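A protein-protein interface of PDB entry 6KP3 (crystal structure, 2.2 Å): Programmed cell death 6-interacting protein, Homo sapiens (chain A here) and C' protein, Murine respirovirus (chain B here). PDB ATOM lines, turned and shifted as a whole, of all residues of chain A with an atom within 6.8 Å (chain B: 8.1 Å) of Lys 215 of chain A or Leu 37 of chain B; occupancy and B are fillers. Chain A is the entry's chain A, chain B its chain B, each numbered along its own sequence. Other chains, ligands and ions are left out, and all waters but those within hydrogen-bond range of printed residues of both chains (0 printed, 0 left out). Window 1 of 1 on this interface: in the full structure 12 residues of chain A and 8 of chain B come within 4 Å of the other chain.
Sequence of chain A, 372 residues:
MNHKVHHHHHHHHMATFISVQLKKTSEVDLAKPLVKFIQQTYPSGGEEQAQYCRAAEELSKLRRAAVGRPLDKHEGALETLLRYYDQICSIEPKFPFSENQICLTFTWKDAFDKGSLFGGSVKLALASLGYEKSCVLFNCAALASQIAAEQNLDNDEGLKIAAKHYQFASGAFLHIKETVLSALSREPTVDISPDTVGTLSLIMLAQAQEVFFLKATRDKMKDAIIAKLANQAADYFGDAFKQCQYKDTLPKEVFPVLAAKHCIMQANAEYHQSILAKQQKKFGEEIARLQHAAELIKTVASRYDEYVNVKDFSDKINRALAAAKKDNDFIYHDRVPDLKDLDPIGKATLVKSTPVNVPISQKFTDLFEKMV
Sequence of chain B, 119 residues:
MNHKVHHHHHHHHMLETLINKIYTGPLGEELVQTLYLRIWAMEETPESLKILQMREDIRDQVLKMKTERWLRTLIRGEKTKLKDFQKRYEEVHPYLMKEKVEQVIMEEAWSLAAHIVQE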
ATOM      1  N   LEU A 153       2.025  33.883 -19.652  1.00  0.00           N
ATOM      2  CA  LEU A 153       0.725  33.790 -18.954  1.00  0.00           C
ATOM      3  C   LEU A 153      -0.273  34.796 -19.524  1.00  0.00           C
ATOM      4  O   LEU A 153      -1.406  34.849 -19.003  1.00  0.00           O
ATOM      5  CB  LEU A 153       0.940  34.067 -17.462  1.00  0.00           C
ATOM      6  CG  LEU A 153       1.931  33.144 -16.755  1.00  0.00           C
ATOM      7  CD1 LEU A 153       1.850  33.319 -15.248  1.00  0.00           C
ATOM      8  CD2 LEU A 153       1.704  31.694 -17.138  1.00  0.00           C
ATOM      9  N   ASP A 156      -2.983  31.807 -23.829  1.00  0.00           N
ATOM     10  CA  ASP A 156      -3.895  30.779 -23.281  1.00  0.00           C
ATOM     11  C   ASP A 156      -3.143  29.451 -23.204  1.00  0.00           C
ATOM     12  O   ASP A 156      -3.299  28.775 -22.189  1.00  0.00           O
ATOM     13  CB  ASP A 156      -5.191  30.680 -24.092  1.00  0.00           C
ATOM     14  CG  ASP A 156      -6.212  29.771 -23.435  1.00  0.00           C
ATOM     15  OD1 ASP A 156      -6.862  30.234 -22.479  1.00  0.00           O
ATOM     16  OD2 ASP A 156      -6.296  28.587 -23.845  1.00  0.00           O
ATOM     17  N   LEU A 159      -0.670  29.374 -20.218  1.00  0.00           N
ATOM     18  CA  LEU A 159      -1.428  29.113 -18.978  1.00  0.00           C
ATOM     19  C   LEU A 159      -1.666  27.602 -18.873  1.00  0.00           C
ATOM     20  O   LEU A 159      -1.409  27.051 -17.803  1.00  0.00           O
ATOM     21  CB  LEU A 159      -2.718  29.922 -19.030  1.00  0.00           C
ATOM     22  CG  LEU A 159      -2.557  31.420 -18.766  1.00  0.00           C
ATOM     23  CD1 LEU A 159      -3.774  32.205 -19.242  1.00  0.00           C
ATOM     24  CD2 LEU A 159      -2.342  31.694 -17.282  1.00  0.00           C
ATOM     25  N   GLU A 210      -2.747  29.642  -8.868  1.00  0.00           N
ATOM     26  CA  GLU A 210      -2.599  31.038  -9.335  1.00  0.00           C
ATOM     27  C   GLU A 210      -2.847  31.032 -10.851  1.00  0.00           C
ATOM     28  O   GLU A 210      -3.548  31.905 -11.347  1.00  0.00           O
ATOM     29  CB  GLU A 210      -1.242  31.625  -8.938  1.00  0.00           C
ATOM     30  CG  GLU A 210      -0.967  32.995  -9.580  1.00  0.00           C
ATOM     31  CD  GLU A 210       0.234  33.735  -9.010  1.00  0.00           C
ATOM     32  OE1 GLU A 210       1.043  33.059  -8.343  1.00  0.00           O
ATOM     33  OE2 GLU A 210       0.357  34.979  -9.226  1.00  0.00           O
ATOM     34  N   VAL A 211      -2.356  30.029 -11.550  1.00  0.00           N
ATOM     35  CA  VAL A 211      -2.521  29.974 -13.025  1.00  0.00           C
ATOM     36  C   VAL A 211      -4.024  29.913 -13.347  1.00  0.00           C
ATOM     37  O   VAL A 211      -4.457  30.663 -14.239  1.00  0.00           O
ATOM     38  CB  VAL A 211      -1.687  28.843 -13.636  1.00  0.00           C
ATOM     39  CG1 VAL A 211      -2.055  28.558 -15.086  1.00  0.00           C
ATOM     40  CG2 VAL A 211      -0.203  29.175 -13.517  1.00  0.00           C
ATOM     41  N   PHE A 212      -4.810  29.127 -12.610  1.00  0.00           N
ATOM     42  CA  PHE A 212      -6.266  28.988 -12.862  1.00  0.00           C
ATOM     43  C   PHE A 212      -6.928  30.333 -12.582  1.00  0.00           C
ATOM     44  O   PHE A 212      -7.775  30.751 -13.359  1.00  0.00           O
ATOM     45  CB  PHE A 212      -6.863  27.845 -12.053  1.00  0.00           C
ATOM     46  CG  PHE A 212      -6.705  26.496 -12.693  1.00  0.00           C
ATOM     47  CD1 PHE A 212      -7.624  26.047 -13.625  1.00  0.00           C
ATOM     48  CD2 PHE A 212      -5.654  25.663 -12.346  1.00  0.00           C
ATOM     49  CE1 PHE A 212      -7.502  24.796 -14.206  1.00  0.00           C
ATOM     50  CE2 PHE A 212      -5.529  24.414 -12.933  1.00  0.00           C
ATOM     51  CZ  PHE A 212      -6.451  23.982 -13.862  1.00  0.00           C
ATOM     52  N   PHE A 213      -6.519  31.018 -11.520  1.00  0.00           N
ATOM     53  CA  PHE A 213      -6.998  32.389 -11.239  1.00  0.00           C
ATOM     54  C   PHE A 213      -6.659  33.320 -12.430  1.00  0.00           C
ATOM     55  O   PHE A 213      -7.517  34.126 -12.806  1.00  0.00           O
ATOM     56  CB  PHE A 213      -6.476  32.893  -9.891  1.00  0.00           C
ATOM     57  CG  PHE A 213      -6.463  34.397  -9.769  1.00  0.00           C
ATOM     58  CD1 PHE A 213      -5.364  35.128 -10.181  1.00  0.00           C
ATOM     59  CD2 PHE A 213      -7.559  35.079  -9.273  1.00  0.00           C
ATOM     60  CE1 PHE A 213      -5.363  36.513 -10.094  1.00  0.00           C
ATOM     61  CE2 PHE A 213      -7.558  36.459  -9.171  1.00  0.00           C
ATOM     62  CZ  PHE A 213      -6.466  37.173  -9.597  1.00  0.00           C
ATOM     63  N   LEU A 214      -5.459  33.239 -13.013  1.00  0.00           N
ATOM     64  CA  LEU A 214      -5.057  34.097 -14.163  1.00  0.00           C
ATOM     65  C   LEU A 214      -5.821  33.704 -15.440  1.00  0.00           C
ATOM     66  O   LEU A 214      -5.988  34.569 -16.309  1.00  0.00           O
ATOM     67  CB  LEU A 214      -3.546  34.006 -14.382  1.00  0.00           C
ATOM     68  CG  LEU A 214      -2.679  34.704 -13.336  1.00  0.00           C
ATOM     69  CD1 LEU A 214      -1.206  34.325 -13.506  1.00  0.00           C
ATOM     70  CD2 LEU A 214      -2.844  36.222 -13.406  1.00  0.00           C
ATOM     71  N   LYS A 215      -6.203  32.441 -15.595  1.00  0.00           N
ATOM     72  CA  LYS A 215      -6.971  31.955 -16.767  1.00  0.00           C
ATOM     73  C   LYS A 215      -8.381  32.533 -16.694  1.00  0.00           C
ATOM     74  O   LYS A 215      -8.937  32.890 -17.746  1.00  0.00           O
ATOM     75  CB  LYS A 215      -7.033  30.429 -16.784  1.00  0.00           C
ATOM     76  CG  LYS A 215      -8.066  29.793 -17.713  1.00  0.00           C
ATOM     77  CD  LYS A 215      -8.002  30.167 -19.170  1.00  0.00           C
ATOM     78  CE  LYS A 215      -9.097  29.474 -19.956  1.00  0.00           C
ATOM     79  NZ  LYS A 215      -9.197  29.930 -21.358  1.00  0.00           N
ATOM     80  N   ALA A 216      -8.920  32.577 -15.484  1.00  0.00           N
ATOM     81  CA  ALA A 216     -10.289  33.018 -15.185  1.00  0.00           C
ATOM     82  C   ALA A 216     -10.346  34.524 -15.407  1.00  0.00           C
ATOM     83  O   ALA A 216     -11.288  34.985 -16.074  1.00  0.00           O
ATOM     84  CB  ALA A 216     -10.673  32.625 -13.779  1.00  0.00           C
ATOM     85  N   THR A 217      -9.336  35.231 -14.908  1.00  0.00           N
ATOM     86  CA  THR A 217      -9.105  36.679 -15.134  1.00  0.00           C
ATOM     87  C   THR A 217      -8.992  36.950 -16.641  1.00  0.00           C
ATOM     88  O   THR A 217      -9.707  37.805 -17.148  1.00  0.00           O
ATOM     89  CB  THR A 217      -7.898  37.177 -14.331  1.00  0.00           C
ATOM     90  OG1 THR A 217      -8.281  37.322 -12.957  1.00  0.00           O
ATOM     91  CG2 THR A 217      -7.391  38.521 -14.815  1.00  0.00           C
ATOM     92  N   ARG A 218      -8.141  36.237 -17.351  1.00  0.00           N
ATOM     93  CA  ARG A 218      -7.913  36.506 -18.786  1.00  0.00           C
ATOM     94  C   ARG A 218      -9.249  36.314 -19.532  1.00  0.00           C
ATOM     95  O   ARG A 218      -9.559  37.144 -20.382  1.00  0.00           O
ATOM     96  CB  ARG A 218      -6.740  35.654 -19.280  1.00  0.00           C
ATOM     97  CG  ARG A 218      -6.379  35.890 -20.739  1.00  0.00           C
ATOM     98  CD  ARG A 218      -5.007  35.349 -21.102  1.00  0.00           C
ATOM     99  NE  ARG A 218      -4.540  35.762 -22.424  1.00  0.00           N
ATOM    100  CZ  ARG A 218      -5.029  35.343 -23.599  1.00  0.00           C
ATOM    101  NH1 ARG A 218      -6.056  34.509 -23.662  1.00  0.00           N
ATOM    102  NH2 ARG A 218      -4.482  35.783 -24.723  1.00  0.00           N
ATOM    103  N   ASP A 219     -10.040  35.299 -19.181  1.00  0.00           N
ATOM    104  CA  ASP A 219     -11.335  34.983 -19.846  1.00  0.00           C
ATOM    105  C   ASP A 219     -12.473  35.907 -19.374  1.00  0.00           C
ATOM    106  O   ASP A 219     -13.561  35.758 -19.905  1.00  0.00           O
ATOM    107  CB  ASP A 219     -11.752  33.527 -19.601  1.00  0.00           C
ATOM    108  CG  ASP A 219     -11.128  32.527 -20.553  1.00  0.00           C
ATOM    109  OD1 ASP A 219     -10.103  32.885 -21.209  1.00  0.00           O
ATOM    110  OD2 ASP A 219     -11.681  31.394 -20.639  1.00  0.00           O
ATOM    111  N   LYS A 220     -12.267  36.809 -18.411  1.00  0.00           N
ATOM    112  CA  LYS A 220     -13.354  37.699 -17.918  1.00  0.00           C
ATOM    113  C   LYS A 220     -14.553  36.830 -17.539  1.00  0.00           C
ATOM    114  O   LYS A 220     -15.654  37.063 -18.057  1.00  0.00           O
ATOM    115  CB  LYS A 220     -13.724  38.743 -18.980  1.00  0.00           C
ATOM    116  CG  LYS A 220     -12.747  39.911 -19.075  1.00  0.00           C
ATOM    117  CD  LYS A 220     -12.790  40.664 -20.379  1.00  0.00           C
ATOM    118  CE  LYS A 220     -11.739  41.754 -20.446  1.00  0.00           C
ATOM    119  NZ  LYS A 220     -11.367  42.074 -21.845  1.00  0.00           N
ATOM    120  N   MET A 221     -14.297  35.821 -16.707  1.00  0.00           N
ATOM    121  CA  MET A 221     -15.307  34.977 -16.025  1.00  0.00           C
ATOM    122  C   MET A 221     -15.909  35.789 -14.879  1.00  0.00           C
ATOM    123  O   MET A 221     -15.387  36.873 -14.562  1.00  0.00           O
ATOM    124  CB  MET A 221     -14.682  33.709 -15.434  1.00  0.00           C
ATOM    125  CG  MET A 221     -13.990  32.855 -16.441  1.00  0.00           C
ATOM    126  SD  MET A 221     -13.697  31.219 -15.760  1.00  0.00           S
ATOM    127  CE  MET A 221     -13.262  30.440 -17.305  1.00  0.00           C
ATOM    128  N   ILE A 225     -16.486  33.433  -9.020  1.00  0.00           N
ATOM    129  CA  ILE A 225     -15.535  32.303  -9.178  1.00  0.00           C
ATOM    130  C   ILE A 225     -14.113  32.869  -9.059  1.00  0.00           C
ATOM    131  O   ILE A 225     -13.311  32.229  -8.378  1.00  0.00           O
ATOM    132  CB  ILE A 225     -15.795  31.517 -10.484  1.00  0.00           C
ATOM    133  CG1 ILE A 225     -15.153  30.127 -10.458  1.00  0.00           C
ATOM    134  CG2 ILE A 225     -15.371  32.287 -11.714  1.00  0.00           C
ATOM    135  CD1 ILE A 225     -15.628  29.225  -9.318  1.00  0.00           C
ATOM    136  N   LEU A 229     -11.299  31.353  -6.609  1.00  0.00           N
ATOM    137  CA  LEU A 229     -10.013  30.856  -7.149  1.00  0.00           C
ATOM    138  C   LEU A 229      -8.866  31.566  -6.429  1.00  0.00           C
ATOM    139  O   LEU A 229      -7.970  30.856  -5.964  1.00  0.00           O
ATOM    140  CB  LEU A 229      -9.959  31.072  -8.664  1.00  0.00           C
ATOM    141  CG  LEU A 229     -10.941  30.218  -9.462  1.00  0.00           C
ATOM    142  CD1 LEU A 229     -10.991  30.635 -10.928  1.00  0.00           C
ATOM    143  CD2 LEU A 229     -10.568  28.758  -9.342  1.00  0.00           C
ATOM    144  N   LEU A 350      -9.046  24.013  -8.083  1.00  0.00           N
ATOM    145  CA  LEU A 350      -8.980  23.516  -9.478  1.00  0.00           C
ATOM    146  C   LEU A 350      -7.719  22.668  -9.674  1.00  0.00           C
ATOM    147  O   LEU A 350      -7.498  22.185 -10.805  1.00  0.00           O
ATOM    148  CB  LEU A 350      -9.062  24.733 -10.406  1.00  0.00           C
ATOM    149  CG  LEU A 350     -10.477  25.063 -10.901  1.00  0.00           C
ATOM    150  CD1 LEU A 350     -10.997  23.959 -11.802  1.00  0.00           C
ATOM    151  CD2 LEU A 350     -11.445  25.298  -9.753  1.00  0.00           C
ATOM    152  N   GLU B  30     -21.329  28.244 -10.895  1.00  0.00           N
ATOM    153  CA  GLU B  30     -20.034  27.790 -10.340  1.00  0.00           C
ATOM    154  C   GLU B  30     -19.650  26.445 -10.956  1.00  0.00           C
ATOM    155  O   GLU B  30     -18.468  26.278 -11.327  1.00  0.00           O
ATOM    156  CB  GLU B  30     -20.093  27.636  -8.820  1.00  0.00           C
ATOM    157  CG  GLU B  30     -18.906  26.861  -8.260  1.00  0.00           C
ATOM    158  CD  GLU B  30     -18.555  27.217  -6.826  1.00  0.00           C
ATOM    159  OE1 GLU B  30     -19.256  28.070  -6.292  1.00  0.00           O
ATOM    160  OE2 GLU B  30     -17.583  26.650  -6.252  1.00  0.00           O
ATOM    161  N   LEU B  31     -20.602  25.515 -11.011  1.00  0.00           N
ATOM    162  CA  LEU B  31     -20.354  24.174 -11.568  1.00  0.00           C
ATOM    163  C   LEU B  31     -19.857  24.315 -13.007  1.00  0.00           C
ATOM    164  O   LEU B  31     -18.829  23.683 -13.310  1.00  0.00           O
ATOM    165  CB  LEU B  31     -21.624  23.337 -11.474  1.00  0.00           C
ATOM    166  CG  LEU B  31     -21.620  22.102 -12.363  1.00  0.00           C
ATOM    167  CD1 LEU B  31     -20.755  21.008 -11.756  1.00  0.00           C
ATOM    168  CD2 LEU B  31     -23.041  21.628 -12.608  1.00  0.00           C
ATOM    169  N   VAL B  32     -20.525  25.096 -13.864  1.00  0.00           N
ATOM    170  CA  VAL B  32     -20.153  25.145 -15.317  1.00  0.00           C
ATOM    171  C   VAL B  32     -18.831  25.903 -15.495  1.00  0.00           C
ATOM    172  O   VAL B  32     -18.147  25.699 -16.517  1.00  0.00           O
ATOM    173  CB  VAL B  32     -21.253  25.734 -16.215  1.00  0.00           C
ATOM    174  CG1 VAL B  32     -22.501  24.854 -16.203  1.00  0.00           C
ATOM    175  CG2 VAL B  32     -21.582  27.175 -15.873  1.00  0.00           C
ATOM    176  N   GLN B  33     -18.467  26.746 -14.537  1.00  0.00           N
ATOM    177  CA  GLN B  33     -17.186  27.485 -14.589  1.00  0.00           C
ATOM    178  C   GLN B  33     -16.071  26.575 -14.065  1.00  0.00           C
ATOM    179  O   GLN B  33     -14.989  26.597 -14.642  1.00  0.00           O
ATOM    180  CB  GLN B  33     -17.346  28.807 -13.839  1.00  0.00           C
ATOM    181  CG  GLN B  33     -18.113  29.824 -14.667  1.00  0.00           C
ATOM    182  CD  GLN B  33     -18.345  31.105 -13.909  1.00  0.00           C
ATOM    183  OE1 GLN B  33     -18.087  32.195 -14.446  1.00  0.00           O
ATOM    184  NE2 GLN B  33     -18.837  30.977 -12.674  1.00  0.00           N
ATOM    185  N   THR B  34     -16.347  25.772 -13.042  1.00  0.00           N
ATOM    186  CA  THR B  34     -15.415  24.732 -12.554  1.00  0.00           C
ATOM    187  C   THR B  34     -15.181  23.690 -13.655  1.00  0.00           C
ATOM    188  O   THR B  34     -13.990  23.355 -13.913  1.00  0.00           O
ATOM    189  CB  THR B  34     -15.897  24.145 -11.227  1.00  0.00           C
ATOM    190  OG1 THR B  34     -15.909  25.247 -10.315  1.00  0.00           O
ATOM    191  CG2 THR B  34     -15.004  23.037 -10.713  1.00  0.00           C
ATOM    192  N   LEU B  35     -16.246  23.252 -14.328  1.00  0.00           N
ATOM    193  CA  LEU B  35     -16.168  22.215 -15.385  1.00  0.00           C
ATOM    194  C   LEU B  35     -15.398  22.732 -16.600  1.00  0.00           C
ATOM    195  O   LEU B  35     -14.656  21.956 -17.196  1.00  0.00           O
ATOM    196  CB  LEU B  35     -17.577  21.771 -15.782  1.00  0.00           C
ATOM    197  CG  LEU B  35     -18.240  20.833 -14.779  1.00  0.00           C
ATOM    198  CD1 LEU B  35     -19.635  20.448 -15.245  1.00  0.00           C
ATOM    199  CD2 LEU B  35     -17.385  19.593 -14.551  1.00  0.00           C
ATOM    200  N   TYR B  36     -15.644  23.962 -17.013  1.00  0.00           N
ATOM    201  CA  TYR B  36     -14.953  24.555 -18.179  1.00  0.00           C
ATOM    202  C   TYR B  36     -13.445  24.619 -17.866  1.00  0.00           C
ATOM    203  O   TYR B  36     -12.661  24.312 -18.778  1.00  0.00           O
ATOM    204  CB  TYR B  36     -15.551  25.920 -18.547  1.00  0.00           C
ATOM    205  CG  TYR B  36     -14.644  26.729 -19.427  1.00  0.00           C
ATOM    206  CD1 TYR B  36     -14.348  26.310 -20.712  1.00  0.00           C
ATOM    207  CD2 TYR B  36     -14.000  27.851 -18.941  1.00  0.00           C
ATOM    208  CE1 TYR B  36     -13.464  27.013 -21.514  1.00  0.00           C
ATOM    209  CE2 TYR B  36     -13.106  28.561 -19.729  1.00  0.00           C
ATOM    210  CZ  TYR B  36     -12.838  28.138 -21.017  1.00  0.00           C
ATOM    211  OH  TYR B  36     -11.977  28.859 -21.788  1.00  0.00           O
ATOM    212  N   LEU B  37     -13.060  25.000 -16.639  1.00  0.00           N
ATOM    213  CA  LEU B  37     -11.627  25.159 -16.241  1.00  0.00           C
ATOM    214  C   LEU B  37     -10.937  23.788 -16.183  1.00  0.00           C
ATOM    215  O   LEU B  37      -9.826  23.666 -16.772  1.00  0.00           O
ATOM    216  CB  LEU B  37     -11.540  25.912 -14.911  1.00  0.00           C
ATOM    217  CG  LEU B  37     -11.935  27.386 -15.012  1.00  0.00           C
ATOM    218  CD1 LEU B  37     -11.936  28.053 -13.658  1.00  0.00           C
ATOM    219  CD2 LEU B  37     -11.016  28.136 -15.954  1.00  0.00           C
ATOM    220  N   ARG B  38     -11.599  22.762 -15.625  1.00  0.00           N
ATOM    221  CA  ARG B  38     -11.057  21.382 -15.625  1.00  0.00           C
ATOM    222  C   ARG B  38     -10.962  20.889 -17.064  1.00  0.00           C
ATOM    223  O   ARG B  38      -9.943  20.294 -17.393  1.00  0.00           O
ATOM    224  CB  ARG B  38     -11.896  20.455 -14.757  1.00  0.00           C
ATOM    225  CG  ARG B  38     -11.996  20.889 -13.303  1.00  0.00           C
ATOM    226  CD  ARG B  38     -12.475  19.775 -12.407  1.00  0.00           C
ATOM    227  NE  ARG B  38     -11.608  18.612 -12.569  1.00  0.00           N
ATOM    228  CZ  ARG B  38     -11.874  17.359 -12.171  1.00  0.00           C
ATOM    229  NH1 ARG B  38     -13.006  17.044 -11.552  1.00  0.00           N
ATOM    230  NH2 ARG B  38     -10.981  16.411 -12.409  1.00  0.00           N
ATOM    231  N   ILE B  39     -11.969  21.116 -17.907  1.00  0.00           N
ATOM    232  CA  ILE B  39     -11.954  20.570 -19.302  1.00  0.00           C
ATOM    233  C   ILE B  39     -10.909  21.334 -20.142  1.00  0.00           C
ATOM    234  O   ILE B  39     -10.196  20.695 -20.945  1.00  0.00           O
ATOM    235  CB  ILE B  39     -13.366  20.602 -19.913  1.00  0.00           C
ATOM    236  CG1 ILE B  39     -14.285  19.612 -19.190  1.00  0.00           C
ATOM    237  CG2 ILE B  39     -13.326  20.344 -21.414  1.00  0.00           C
ATOM    238  CD1 ILE B  39     -15.753  19.752 -19.546  1.00  0.00           C
ATOM    239  N   TRP B  40     -10.829  22.653 -19.970  1.00  0.00           N
ATOM    240  CA  TRP B  40      -9.734  23.512 -20.498  1.00  0.00           C
ATOM    241  C   TRP B  40      -8.360  22.885 -20.178  1.00  0.00           C
ATOM    242  O   TRP B  40      -7.564  22.669 -21.120  1.00  0.00           O
ATOM    243  CB  TRP B  40      -9.853  24.942 -19.941  1.00  0.00           C
ATOM    244  CG  TRP B  40      -8.652  25.777 -20.272  1.00  0.00           C
ATOM    245  CD1 TRP B  40      -8.324  26.278 -21.496  1.00  0.00           C
ATOM    246  CD2 TRP B  40      -7.585  26.147 -19.388  1.00  0.00           C
ATOM    247  NE1 TRP B  40      -7.141  26.955 -21.424  1.00  0.00           N
ATOM    248  CE2 TRP B  40      -6.668  26.907 -20.146  1.00  0.00           C
ATOM    249  CE3 TRP B  40      -7.317  25.930 -18.030  1.00  0.00           C
ATOM    250  CZ2 TRP B  40      -5.505  27.450 -19.595  1.00  0.00           C
ATOM    251  CZ3 TRP B  40      -6.168  26.459 -17.486  1.00  0.00           C
ATOM    252  CH2 TRP B  40      -5.272  27.201 -18.262  1.00  0.00           C
ATOM    253  N   ALA B  41      -8.122  22.528 -18.917  1.00  0.00           N
ATOM    254  CA  ALA B  41      -6.785  22.175 -18.385  1.00  0.00           C
ATOM    255  C   ALA B  41      -6.328  20.800 -18.865  1.00  0.00           C
ATOM    256  O   ALA B  41      -5.122  20.605 -18.998  1.00  0.00           O
ATOM    257  CB  ALA B  41      -6.788  22.199 -16.882  1.00  0.00           C
ATOM    258  N   MET B  42      -7.260  19.895 -19.123  1.00  0.00           N
ATOM    259  CA  MET B  42      -6.952  18.468 -19.331  1.00  0.00           C
ATOM    260  C   MET B  42      -6.285  18.295 -20.693  1.00  0.00           C
ATOM    261  O   MET B  42      -6.381  19.236 -21.526  1.00  0.00           O
ATOM    262  CB  MET B  42      -8.209  17.596 -19.230  1.00  0.00           C
ATOM    263  CG  MET B  42      -9.275  17.818 -20.322  1.00  0.00           C
ATOM    264  SD  MET B  42     -10.807  16.855 -19.960  1.00  0.00           S
ATOM    265  CE  MET B  42     -10.528  15.435 -21.017  1.00  0.00           C
ATOM    266  N   LEU B  52     -14.842  22.873 -25.846  1.00  0.00           N
ATOM    267  CA  LEU B  52     -14.092  24.165 -25.752  1.00  0.00           C
ATOM    268  C   LEU B  52     -14.444  25.073 -26.948  1.00  0.00           C
ATOM    269  O   LEU B  52     -14.517  26.300 -26.755  1.00  0.00           O
ATOM    270  CB  LEU B  52     -12.575  23.903 -25.654  1.00  0.00           C
ATOM    271  CG  LEU B  52     -12.076  23.330 -24.322  1.00  0.00           C
ATOM    272  CD1 LEU B  52     -10.591  22.998 -24.367  1.00  0.00           C
ATOM    273  CD2 LEU B  52     -12.352  24.296 -23.189  1.00  0.00           C
ATOM    274  N   ARG B  59     -22.199  25.727 -24.345  1.00  0.00           N
ATOM    275  CA  ARG B  59     -21.330  24.917 -23.441  1.00  0.00           C
ATOM    276  C   ARG B  59     -21.975  24.839 -22.040  1.00  0.00           C
ATOM    277  O   ARG B  59     -22.049  23.726 -21.506  1.00  0.00           O
ATOM    278  CB  ARG B  59     -19.896  25.465 -23.409  1.00  0.00           C
ATOM    279  CG  ARG B  59     -18.941  24.631 -22.568  1.00  0.00           C
ATOM    280  CD  ARG B  59     -17.544  25.189 -22.387  1.00  0.00           C
ATOM    281  NE  ARG B  59     -17.507  26.633 -22.220  1.00  0.00           N
ATOM    282  CZ  ARG B  59     -17.077  27.489 -23.150  1.00  0.00           C
ATOM    283  NH1 ARG B  59     -16.628  27.050 -24.318  1.00  0.00           N
ATOM    284  NH2 ARG B  59     -17.091  28.784 -22.902  1.00  0.00           N
ATOM    285  N   LEU B  63     -23.092  21.233 -20.293  1.00  0.00           N
ATOM    286  CA  LEU B  63     -22.424  20.801 -19.038  1.00  0.00           C
ATOM    287  C   LEU B  63     -23.476  20.628 -17.929  1.00  0.00           C
ATOM    288  O   LEU B  63     -23.353  19.669 -17.127  1.00  0.00           O
ATOM    289  CB  LEU B  63     -21.352  21.818 -18.649  1.00  0.00           C
ATOM    290  CG  LEU B  63     -20.130  21.885 -19.566  1.00  0.00           C
ATOM    291  CD1 LEU B  63     -19.106  22.854 -18.999  1.00  0.00           C
ATOM    292  CD2 LEU B  63     -19.487  20.524 -19.787  1.00  0.00           C
ATOM    293  N   VAL B 104     -14.595  13.524 -15.677  1.00  0.00           N
ATOM    294  CA  VAL B 104     -14.488  14.853 -15.004  1.00  0.00           C
ATOM    295  C   VAL B 104     -15.881  15.292 -14.526  1.00  0.00           C
ATOM    296  O   VAL B 104     -15.993  15.800 -13.376  1.00  0.00           O
ATOM    297  CB  VAL B 104     -13.841  15.901 -15.933  1.00  0.00           C
ATOM    298  CG1 VAL B 104     -14.193  17.312 -15.511  1.00  0.00           C
ATOM    299  CG2 VAL B 104     -12.331  15.699 -15.974  1.00  0.00           C
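The side-chain carboxylate of Asp 156 of chain A sits at hydrogen-bond distance from the indole nitrogen of Trp 40 of chain B (3.0 Å).
The side-chain amino group (NZ) of Lys 215 of chain A lies within hydrogen-bond range of the side-chain hydroxyl (OH) of Tyr 36 of chain B, at 3.0 Å.
OD2 of Asp 219 of chain A sits at hydrogen-bond distance from OH of Tyr 36 of chain B, 2.8 Å away.
The side-chain amino group (NZ) of Lys 215 of chain A lies within salt-bridge range of the side-chain carboxylate (OD1) of Asp 156 of chain A.
The side-chain amino group (NZ) of Lys 215 of chain A lies within salt-bridge range of the side-chain carboxylate (OD2) of Asp 219 of chain A, at 3.0 Å.
O of Ala 216 of chain A is in hydrogen-bond range of N of Met 221 of chain A (3.2 Å).
The backbone carbonyl oxygen of Glu 30 of chain B is in hydrogen-bond range of the side-chain hydroxyl of Thr 34 of chain B (2.9 Å).
Leu 159 of chain A touches Trp 40 of chain B (C to CH2, 3.7 Å).
Phe 212 of chain A touches Leu 37 of chain B.
Leu 37 of chain B touches Lys 215 of chain A (CD2 to CG, 3.8 Å).
CE of Lys 215 of chain A touches NE1 of Trp 40 of chain B, 3.5 Å away.
Met 221 of chain A touches Gln 33 of chain B.
Leu 37 of chain B touches Met 221 of chain A (CD2 to CE, 3.5 Å).
Ile 225 of chain A touches Gln 33 of chain B.
Leu 229 of chain A touches Leu 37 of chain B (CD1 to CD1, 3.9 Å).
Leu 37 of chain B touches Leu 350 of chain A (CB to CD1, 3.7 Å).
Leu 350 of chain A touches Arg 38 of chain B.
Lys 215 of chain A touches three residues of chain B.
Of the printed residues of chain A, Leu 37 of chain B touches Phe 212, Lys 215, Met 221, Leu 229 and Leu 350.
No residue of chain B comes within 4 Å of Ala 216 of chain A.
Printed residues of chain B within 4 Å of Asp 219 of chain A: Tyr 36.
Of the printed residues of chain A, Trp 40 of chain B touches Asp 156, Leu 159, Phe 212 and Lys 215.
Of the printed residues of chain A, Thr 34 of chain B touches Leu 350.
The nearest residue of chain B that does not touch Lys 215 of chain A is Leu 52 of chain B (6.7 Å).
The nearest residue of chain A that does not touch Leu 37 of chain B is Ala 216 of chain A (4.7 Å).
Hydrophobic or aromatic side chains of chain A within 4 Å of the printed part of chain B: Leu 159, Phe 212, Met 221, Ile 225, Leu 229 and Leu 350.
Of the 17 printed residues of chain B, 7 touch a printed residue of chain A.
Hydrophobic or aromatic side chains of chain B within 4 Å of the printed part of chain A: Tyr 36, Leu 37, Trp 40 and Ala 41.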
